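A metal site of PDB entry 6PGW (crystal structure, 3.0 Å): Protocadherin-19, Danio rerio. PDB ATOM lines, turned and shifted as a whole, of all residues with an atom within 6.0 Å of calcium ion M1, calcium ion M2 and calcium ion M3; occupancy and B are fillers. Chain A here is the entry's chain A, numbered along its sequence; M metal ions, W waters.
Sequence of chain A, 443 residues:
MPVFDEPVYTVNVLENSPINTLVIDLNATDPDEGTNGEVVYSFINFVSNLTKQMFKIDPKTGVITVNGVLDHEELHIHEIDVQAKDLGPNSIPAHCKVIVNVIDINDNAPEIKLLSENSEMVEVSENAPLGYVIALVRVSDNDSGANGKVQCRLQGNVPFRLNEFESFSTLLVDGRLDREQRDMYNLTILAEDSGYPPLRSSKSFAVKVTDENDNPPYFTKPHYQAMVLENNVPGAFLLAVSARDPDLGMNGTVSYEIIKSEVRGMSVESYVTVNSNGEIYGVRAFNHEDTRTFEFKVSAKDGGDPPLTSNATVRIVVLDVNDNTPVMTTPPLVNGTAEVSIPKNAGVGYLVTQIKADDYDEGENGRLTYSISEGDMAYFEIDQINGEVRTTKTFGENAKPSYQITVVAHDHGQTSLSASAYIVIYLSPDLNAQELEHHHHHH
OD1 of Asp 302 sits at hydrogen-bond distance from N of Leu 308, at 2.7 Å. The side-chain amide nitrogen of Asn 127 sits close to the side-chain carboxylate of Asp 214 (3.3 Å). The backbone NH of Arg 179 lies close to the side-chain carboxylate of Glu 126, 3.0 Å away. OD2 of Asp 211 lies within hydrogen-bond range of N of Leu 248, at 2.7 Å.
Six residues have an atom within 4 Å of calcium ion M1: Glu 126, Glu 180, Asp 211, Glu 212, Asp 214 and Asp 247.
Six residues have an atom within 4 Å of calcium ion M3: Asn 213, Asn 215, Asp 245, Asp 247, Asn 251 and Asp 302.
Calcium ion M1 is bound by OE1 of Glu 126 (2.3 Å). Calcium ion M1 is bound by OD1 of Asp 247, at 2.3 Å. The side-chain carboxylate (OE1) of Glu 180 binds calcium ion M1 (2.3 Å). O of Glu 212 binds calcium ion M1 (2.3 Å). OD1 of Asp 214 is bound to calcium ion M1, at 2.4 Å. Calcium ion M1 is bound by OD1 of Asp 211 (2.4 Å). Slightly farther from calcium ion M1 lies the side-chain carboxylate (OE2) of Glu 180 (3.1 Å).
Calcium ion M2 is bound by OD2 of Asp 214 (2.3 Å), OE2 of Glu 126 (2.3 Å), OE2 of Glu 180 (2.3 Å), water W1 (2.3 Å), water W2 (2.3 Å) and OD1 of Asp 178 (2.3 Å).
OD2 of Asp 302 is bound to calcium ion M3. The backbone carbonyl oxygen (O) of Asn 215 binds calcium ion M3. O of Asn 251 is bound to calcium ion M3, 2.3 Å away. OD2 of Asp 245 binds calcium ion M3, 2.3 Å away. The side-chain carboxylate (OD2) of Asp 247 is bound to calcium ion M3. OD1 of Asn 213 is bound to calcium ion M3 (2.3 Å). Slightly farther from calcium ion M3 lies the side-chain carboxylate (OD1) of Asp 245 (3.0 Å).
Water W1 bridges the side-chain carboxylate (OD2) of Asp 178 (3.3 Å) and the side-chain amide oxygen (OD1) of Asn 215 (3.5 Å).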
ATOM      1  N   GLU A 126      23.761   8.990  21.814  1.00  0.00           N
ATOM      2  CA  GLU A 126      25.142   9.175  21.332  1.00  0.00           C
ATOM      3  C   GLU A 126      25.195   9.896  20.027  1.00  0.00           C
ATOM      4  O   GLU A 126      24.356   9.661  19.151  1.00  0.00           O
ATOM      5  CB  GLU A 126      25.806   7.857  21.022  1.00  0.00           C
ATOM      6  CG  GLU A 126      25.786   6.811  22.085  1.00  0.00           C
ATOM      7  CD  GLU A 126      26.549   5.621  21.642  1.00  0.00           C
ATOM      8  OE1 GLU A 126      25.933   4.634  21.246  1.00  0.00           O
ATOM      9  OE2 GLU A 126      27.770   5.738  21.587  1.00  0.00           O
ATOM     10  N   ASN A 127      26.246  10.680  19.832  1.00  0.00           N
ATOM     11  CA  ASN A 127      26.463  11.436  18.602  1.00  0.00           C
ATOM     12  C   ASN A 127      25.146  11.967  18.020  1.00  0.00           C
ATOM     13  O   ASN A 127      24.926  11.944  16.804  1.00  0.00           O
ATOM     14  CB  ASN A 127      27.265  10.590  17.552  1.00  0.00           C
ATOM     15  CG  ASN A 127      26.619   9.234  17.232  1.00  0.00           C
ATOM     16  OD1 ASN A 127      25.429   9.151  16.931  1.00  0.00           O
ATOM     17  ND2 ASN A 127      27.407   8.161  17.295  1.00  0.00           N
ATOM     18  N   LEU A 177      29.203  13.168  20.865  1.00  0.00           N
ATOM     19  CA  LEU A 177      29.037  12.322  22.043  1.00  0.00           C
ATOM     20  C   LEU A 177      29.232  10.879  21.696  1.00  0.00           C
ATOM     21  O   LEU A 177      28.564  10.348  20.806  1.00  0.00           O
ATOM     22  CB  LEU A 177      27.664  12.514  22.682  1.00  0.00           C
ATOM     23  CG  LEU A 177      27.173  13.948  22.832  1.00  0.00           C
ATOM     24  CD1 LEU A 177      25.644  13.976  22.888  1.00  0.00           C
ATOM     25  CD2 LEU A 177      27.801  14.597  24.073  1.00  0.00           C
ATOM     26  N   ASP A 178      30.135  10.229  22.418  1.00  0.00           N
ATOM     27  CA  ASP A 178      30.366   8.809  22.298  1.00  0.00           C
ATOM     28  C   ASP A 178      30.117   8.181  23.656  1.00  0.00           C
ATOM     29  O   ASP A 178      30.763   8.552  24.634  1.00  0.00           O
ATOM     30  CB  ASP A 178      31.792   8.561  21.848  1.00  0.00           C
ATOM     31  CG  ASP A 178      32.020   7.146  21.377  1.00  0.00           C
ATOM     32  OD1 ASP A 178      31.071   6.324  21.334  1.00  0.00           O
ATOM     33  OD2 ASP A 178      33.178   6.850  21.030  1.00  0.00           O
ATOM     34  N   ARG A 179      29.145   7.250  23.729  1.00  0.00           N
ATOM     35  CA  ARG A 179      28.826   6.530  24.966  1.00  0.00           C
ATOM     36  C   ARG A 179      29.979   5.622  25.395  1.00  0.00           C
ATOM     37  O   ARG A 179      30.344   5.559  26.582  1.00  0.00           O
ATOM     38  CB  ARG A 179      27.557   5.693  24.789  1.00  0.00           C
ATOM     39  CG  ARG A 179      27.323   4.694  25.908  1.00  0.00           C
ATOM     40  CD  ARG A 179      25.867   4.486  26.197  1.00  0.00           C
ATOM     41  NE  ARG A 179      25.682   3.791  27.482  1.00  0.00           N
ATOM     42  CZ  ARG A 179      25.201   4.351  28.606  1.00  0.00           C
ATOM     43  NH1 ARG A 179      25.084   3.599  29.687  1.00  0.00           N
ATOM     44  NH2 ARG A 179      24.853   5.646  28.669  1.00  0.00           N
ATOM     45  N   GLU A 180      30.558   4.935  24.407  1.00  0.00           N
ATOM     46  CA  GLU A 180      31.687   4.048  24.636  1.00  0.00           C
ATOM     47  C   GLU A 180      32.841   4.789  25.318  1.00  0.00           C
ATOM     48  O   GLU A 180      33.610   4.175  26.039  1.00  0.00           O
ATOM     49  CB  GLU A 180      32.144   3.397  23.326  1.00  0.00           C
ATOM     50  CG  GLU A 180      31.248   2.231  22.869  1.00  0.00           C
ATOM     51  CD  GLU A 180      29.868   2.675  22.365  1.00  0.00           C
ATOM     52  OE1 GLU A 180      28.864   1.944  22.555  1.00  0.00           O
ATOM     53  OE2 GLU A 180      29.778   3.761  21.802  1.00  0.00           O
ATOM     54  N   ASP A 211      22.400   4.920  24.761  1.00  0.00           N
ATOM     55  CA  ASP A 211      23.183   4.081  23.853  1.00  0.00           C
ATOM     56  C   ASP A 211      22.524   3.940  22.497  1.00  0.00           C
ATOM     57  O   ASP A 211      21.308   3.863  22.379  1.00  0.00           O
ATOM     58  CB  ASP A 211      23.381   2.683  24.458  1.00  0.00           C
ATOM     59  CG  ASP A 211      24.378   1.810  23.643  1.00  0.00           C
ATOM     60  OD1 ASP A 211      25.498   2.299  23.222  1.00  0.00           O
ATOM     61  OD2 ASP A 211      24.018   0.624  23.424  1.00  0.00           O
ATOM     62  N   GLU A 212      23.365   3.902  21.484  1.00  0.00           N
ATOM     63  CA  GLU A 212      22.994   3.547  20.152  1.00  0.00           C
ATOM     64  C   GLU A 212      23.803   2.319  19.767  1.00  0.00           C
ATOM     65  O   GLU A 212      24.895   2.048  20.349  1.00  0.00           O
ATOM     66  CB  GLU A 212      23.305   4.704  19.192  1.00  0.00           C
ATOM     67  CG  GLU A 212      22.192   5.720  19.047  1.00  0.00           C
ATOM     68  CD  GLU A 212      20.862   5.082  18.678  1.00  0.00           C
ATOM     69  OE1 GLU A 212      19.813   5.646  19.056  1.00  0.00           O
ATOM     70  OE2 GLU A 212      20.862   3.997  18.034  1.00  0.00           O
ATOM     71  N   ASN A 213      23.244   1.557  18.836  1.00  0.00           N
ATOM     72  CA  ASN A 213      23.885   0.396  18.282  1.00  0.00           C
ATOM     73  C   ASN A 213      24.739   0.939  17.158  1.00  0.00           C
ATOM     74  O   ASN A 213      24.375   0.858  16.017  1.00  0.00           O
ATOM     75  CB  ASN A 213      22.796  -0.543  17.733  1.00  0.00           C
ATOM     76  CG  ASN A 213      23.316  -1.940  17.448  1.00  0.00           C
ATOM     77  OD1 ASN A 213      24.227  -2.444  18.103  1.00  0.00           O
ATOM     78  ND2 ASN A 213      22.705  -2.602  16.458  1.00  0.00           N
ATOM     79  N   ASP A 214      25.828   1.606  17.486  1.00  0.00           N
ATOM     80  CA  ASP A 214      26.641   2.254  16.452  1.00  0.00           C
ATOM     81  C   ASP A 214      27.897   1.476  16.115  1.00  0.00           C
ATOM     82  O   ASP A 214      28.596   1.836  15.161  1.00  0.00           O
ATOM     83  CB  ASP A 214      26.942   3.736  16.767  1.00  0.00           C
ATOM     84  CG  ASP A 214      27.363   3.980  18.199  1.00  0.00           C
ATOM     85  OD1 ASP A 214      27.157   3.110  19.100  1.00  0.00           O
ATOM     86  OD2 ASP A 214      27.859   5.078  18.400  1.00  0.00           O
ATOM     87  N   ASN A 215      28.159   0.387  16.845  1.00  0.00           N
ATOM     88  CA  ASN A 215      29.316  -0.499  16.599  1.00  0.00           C
ATOM     89  C   ASN A 215      28.846  -1.918  16.548  1.00  0.00           C
ATOM     90  O   ASN A 215      27.945  -2.262  17.277  1.00  0.00           O
ATOM     91  CB  ASN A 215      30.266  -0.427  17.753  1.00  0.00           C
ATOM     92  CG  ASN A 215      30.724   0.961  18.038  1.00  0.00           C
ATOM     93  OD1 ASN A 215      31.252   1.219  19.100  1.00  0.00           O
ATOM     94  ND2 ASN A 215      30.543   1.863  17.087  1.00  0.00           N
ATOM     95  N   PRO A 216      29.509  -2.777  15.740  1.00  0.00           N
ATOM     96  CA  PRO A 216      29.225  -4.208  15.764  1.00  0.00           C
ATOM     97  C   PRO A 216      30.203  -4.991  16.685  1.00  0.00           C
ATOM     98  O   PRO A 216      31.123  -4.376  17.280  1.00  0.00           O
ATOM     99  CB  PRO A 216      29.445  -4.604  14.304  1.00  0.00           C
ATOM    100  CG  PRO A 216      30.607  -3.762  13.897  1.00  0.00           C
ATOM    101  CD  PRO A 216      30.516  -2.471  14.702  1.00  0.00           C
ATOM    102  N   PRO A 217      30.026  -6.331  16.777  1.00  0.00           N
ATOM    103  CA  PRO A 217      30.997  -7.149  17.519  1.00  0.00           C
ATOM    104  C   PRO A 217      32.295  -7.258  16.753  1.00  0.00           C
ATOM    105  O   PRO A 217      32.309  -7.674  15.591  1.00  0.00           O
ATOM    106  CB  PRO A 217      30.313  -8.519  17.654  1.00  0.00           C
ATOM    107  CG  PRO A 217      28.913  -8.340  17.171  1.00  0.00           C
ATOM    108  CD  PRO A 217      28.920  -7.160  16.245  1.00  0.00           C
ATOM    109  N   ASP A 245      31.202  -6.720  21.543  1.00  0.00           N
ATOM    110  CA  ASP A 245      30.501  -5.567  21.078  1.00  0.00           C
ATOM    111  C   ASP A 245      30.412  -4.562  22.215  1.00  0.00           C
ATOM    112  O   ASP A 245      29.946  -4.888  23.319  1.00  0.00           O
ATOM    113  CB  ASP A 245      29.131  -5.969  20.614  1.00  0.00           C
ATOM    114  CG  ASP A 245      28.389  -4.840  19.972  1.00  0.00           C
ATOM    115  OD1 ASP A 245      28.258  -3.770  20.618  1.00  0.00           O
ATOM    116  OD2 ASP A 245      27.899  -5.027  18.855  1.00  0.00           O
ATOM    117  N   PRO A 246      30.838  -3.323  21.955  1.00  0.00           N
ATOM    118  CA  PRO A 246      30.906  -2.339  23.039  1.00  0.00           C
ATOM    119  C   PRO A 246      29.581  -1.703  23.448  1.00  0.00           C
ATOM    120  O   PRO A 246      29.533  -1.020  24.442  1.00  0.00           O
ATOM    121  CB  PRO A 246      31.865  -1.284  22.501  1.00  0.00           C
ATOM    122  CG  PRO A 246      31.770  -1.401  21.027  1.00  0.00           C
ATOM    123  CD  PRO A 246      31.384  -2.802  20.697  1.00  0.00           C
ATOM    124  N   ASP A 247      28.506  -1.948  22.692  1.00  0.00           N
ATOM    125  CA  ASP A 247      27.218  -1.365  23.019  1.00  0.00           C
ATOM    126  C   ASP A 247      26.545  -1.973  24.220  1.00  0.00           C
ATOM    127  O   ASP A 247      26.989  -2.986  24.772  1.00  0.00           O
ATOM    128  CB  ASP A 247      26.279  -1.517  21.857  1.00  0.00           C
ATOM    129  CG  ASP A 247      26.763  -0.855  20.669  1.00  0.00           C
ATOM    130  OD1 ASP A 247      27.179   0.323  20.794  1.00  0.00           O
ATOM    131  OD2 ASP A 247      26.781  -1.485  19.615  1.00  0.00           O
ATOM    132  N   LEU A 248      25.446  -1.340  24.590  1.00  0.00           N
ATOM    133  CA  LEU A 248      24.670  -1.738  25.743  1.00  0.00           C
ATOM    134  C   LEU A 248      23.664  -2.797  25.412  1.00  0.00           C
ATOM    135  O   LEU A 248      22.913  -2.689  24.446  1.00  0.00           O
ATOM    136  CB  LEU A 248      23.963  -0.542  26.351  1.00  0.00           C
ATOM    137  CG  LEU A 248      24.621  -0.039  27.614  1.00  0.00           C
ATOM    138  CD1 LEU A 248      26.060   0.403  27.369  1.00  0.00           C
ATOM    139  CD2 LEU A 248      23.771   1.098  28.197  1.00  0.00           C
ATOM    140  N   MET A 250      21.368  -5.659  24.277  1.00  0.00           N
ATOM    141  CA  MET A 250      21.014  -6.348  23.076  1.00  0.00           C
ATOM    142  C   MET A 250      21.870  -5.845  21.973  1.00  0.00           C
ATOM    143  O   MET A 250      22.246  -6.596  21.075  1.00  0.00           O
ATOM    144  CB  MET A 250      19.619  -5.990  22.716  1.00  0.00           C
ATOM    145  CG  MET A 250      18.624  -6.281  23.813  1.00  0.00           C
ATOM    146  SD  MET A 250      17.659  -7.724  23.402  1.00  0.00           S
ATOM    147  CE  MET A 250      16.578  -7.066  22.123  1.00  0.00           C
ATOM    148  N   ASN A 251      22.119  -4.548  21.977  1.00  0.00           N
ATOM    149  CA  ASN A 251      22.922  -3.944  20.935  1.00  0.00           C
ATOM    150  C   ASN A 251      24.305  -4.538  20.932  1.00  0.00           C
ATOM    151  O   ASN A 251      24.989  -4.577  19.903  1.00  0.00           O
ATOM    152  CB  ASN A 251      22.979  -2.416  21.097  1.00  0.00           C
ATOM    153  CG  ASN A 251      21.732  -1.699  20.563  1.00  0.00           C
ATOM    154  OD1 ASN A 251      21.619  -0.486  20.680  1.00  0.00           O
ATOM    155  ND2 ASN A 251      20.814  -2.449  19.942  1.00  0.00           N
ATOM    156  N   GLY A 252      24.723  -5.001  22.109  1.00  0.00           N
ATOM    157  CA  GLY A 252      26.048  -5.536  22.329  1.00  0.00           C
ATOM    158  C   GLY A 252      26.184  -7.016  22.702  1.00  0.00           C
ATOM    159  O   GLY A 252      27.252  -7.461  23.091  1.00  0.00           O
ATOM    160  N   ASP A 302      24.227  -8.953  16.637  1.00  0.00           N
ATOM    161  CA  ASP A 302      23.759  -8.388  17.910  1.00  0.00           C
ATOM    162  C   ASP A 302      22.342  -7.908  17.780  1.00  0.00           C
ATOM    163  O   ASP A 302      21.913  -7.571  16.689  1.00  0.00           O
ATOM    164  CB  ASP A 302      24.608  -7.194  18.270  1.00  0.00           C
ATOM    165  CG  ASP A 302      24.615  -6.151  17.178  1.00  0.00           C
ATOM    166  OD1 ASP A 302      24.127  -6.420  16.063  1.00  0.00           O
ATOM    167  OD2 ASP A 302      25.112  -5.085  17.411  1.00  0.00           O
ATOM    168  N   LEU A 308      23.567  -5.682  13.574  1.00  0.00           N
ATOM    169  CA  LEU A 308      24.812  -5.546  12.823  1.00  0.00           C
ATOM    170  C   LEU A 308      25.689  -6.803  12.865  1.00  0.00           C
ATOM    171  O   LEU A 308      25.581  -7.606  13.786  1.00  0.00           O
ATOM    172  CB  LEU A 308      25.592  -4.349  13.349  1.00  0.00           C
ATOM    173  CG  LEU A 308      24.867  -3.034  13.101  1.00  0.00           C
ATOM    174  CD1 LEU A 308      25.646  -1.938  13.771  1.00  0.00           C
ATOM    175  CD2 LEU A 308      24.682  -2.772  11.611  1.00  0.00           C
HETATM  176 CA    CA M   1      26.940   2.565  21.377  1.00  0.00          CA
HETATM  177 CA    CA M   2      29.425   5.237  20.073  1.00  0.00          CA
HETATM  178 CA    CA M   3      26.308  -3.407  18.417  1.00  0.00          CA
HETATM  179  O   HOH W   1      31.517   4.666  19.267  1.00  0.00           O
HETATM  180  O   HOH W   2      29.664   6.632  18.226  1.00  0.00           O
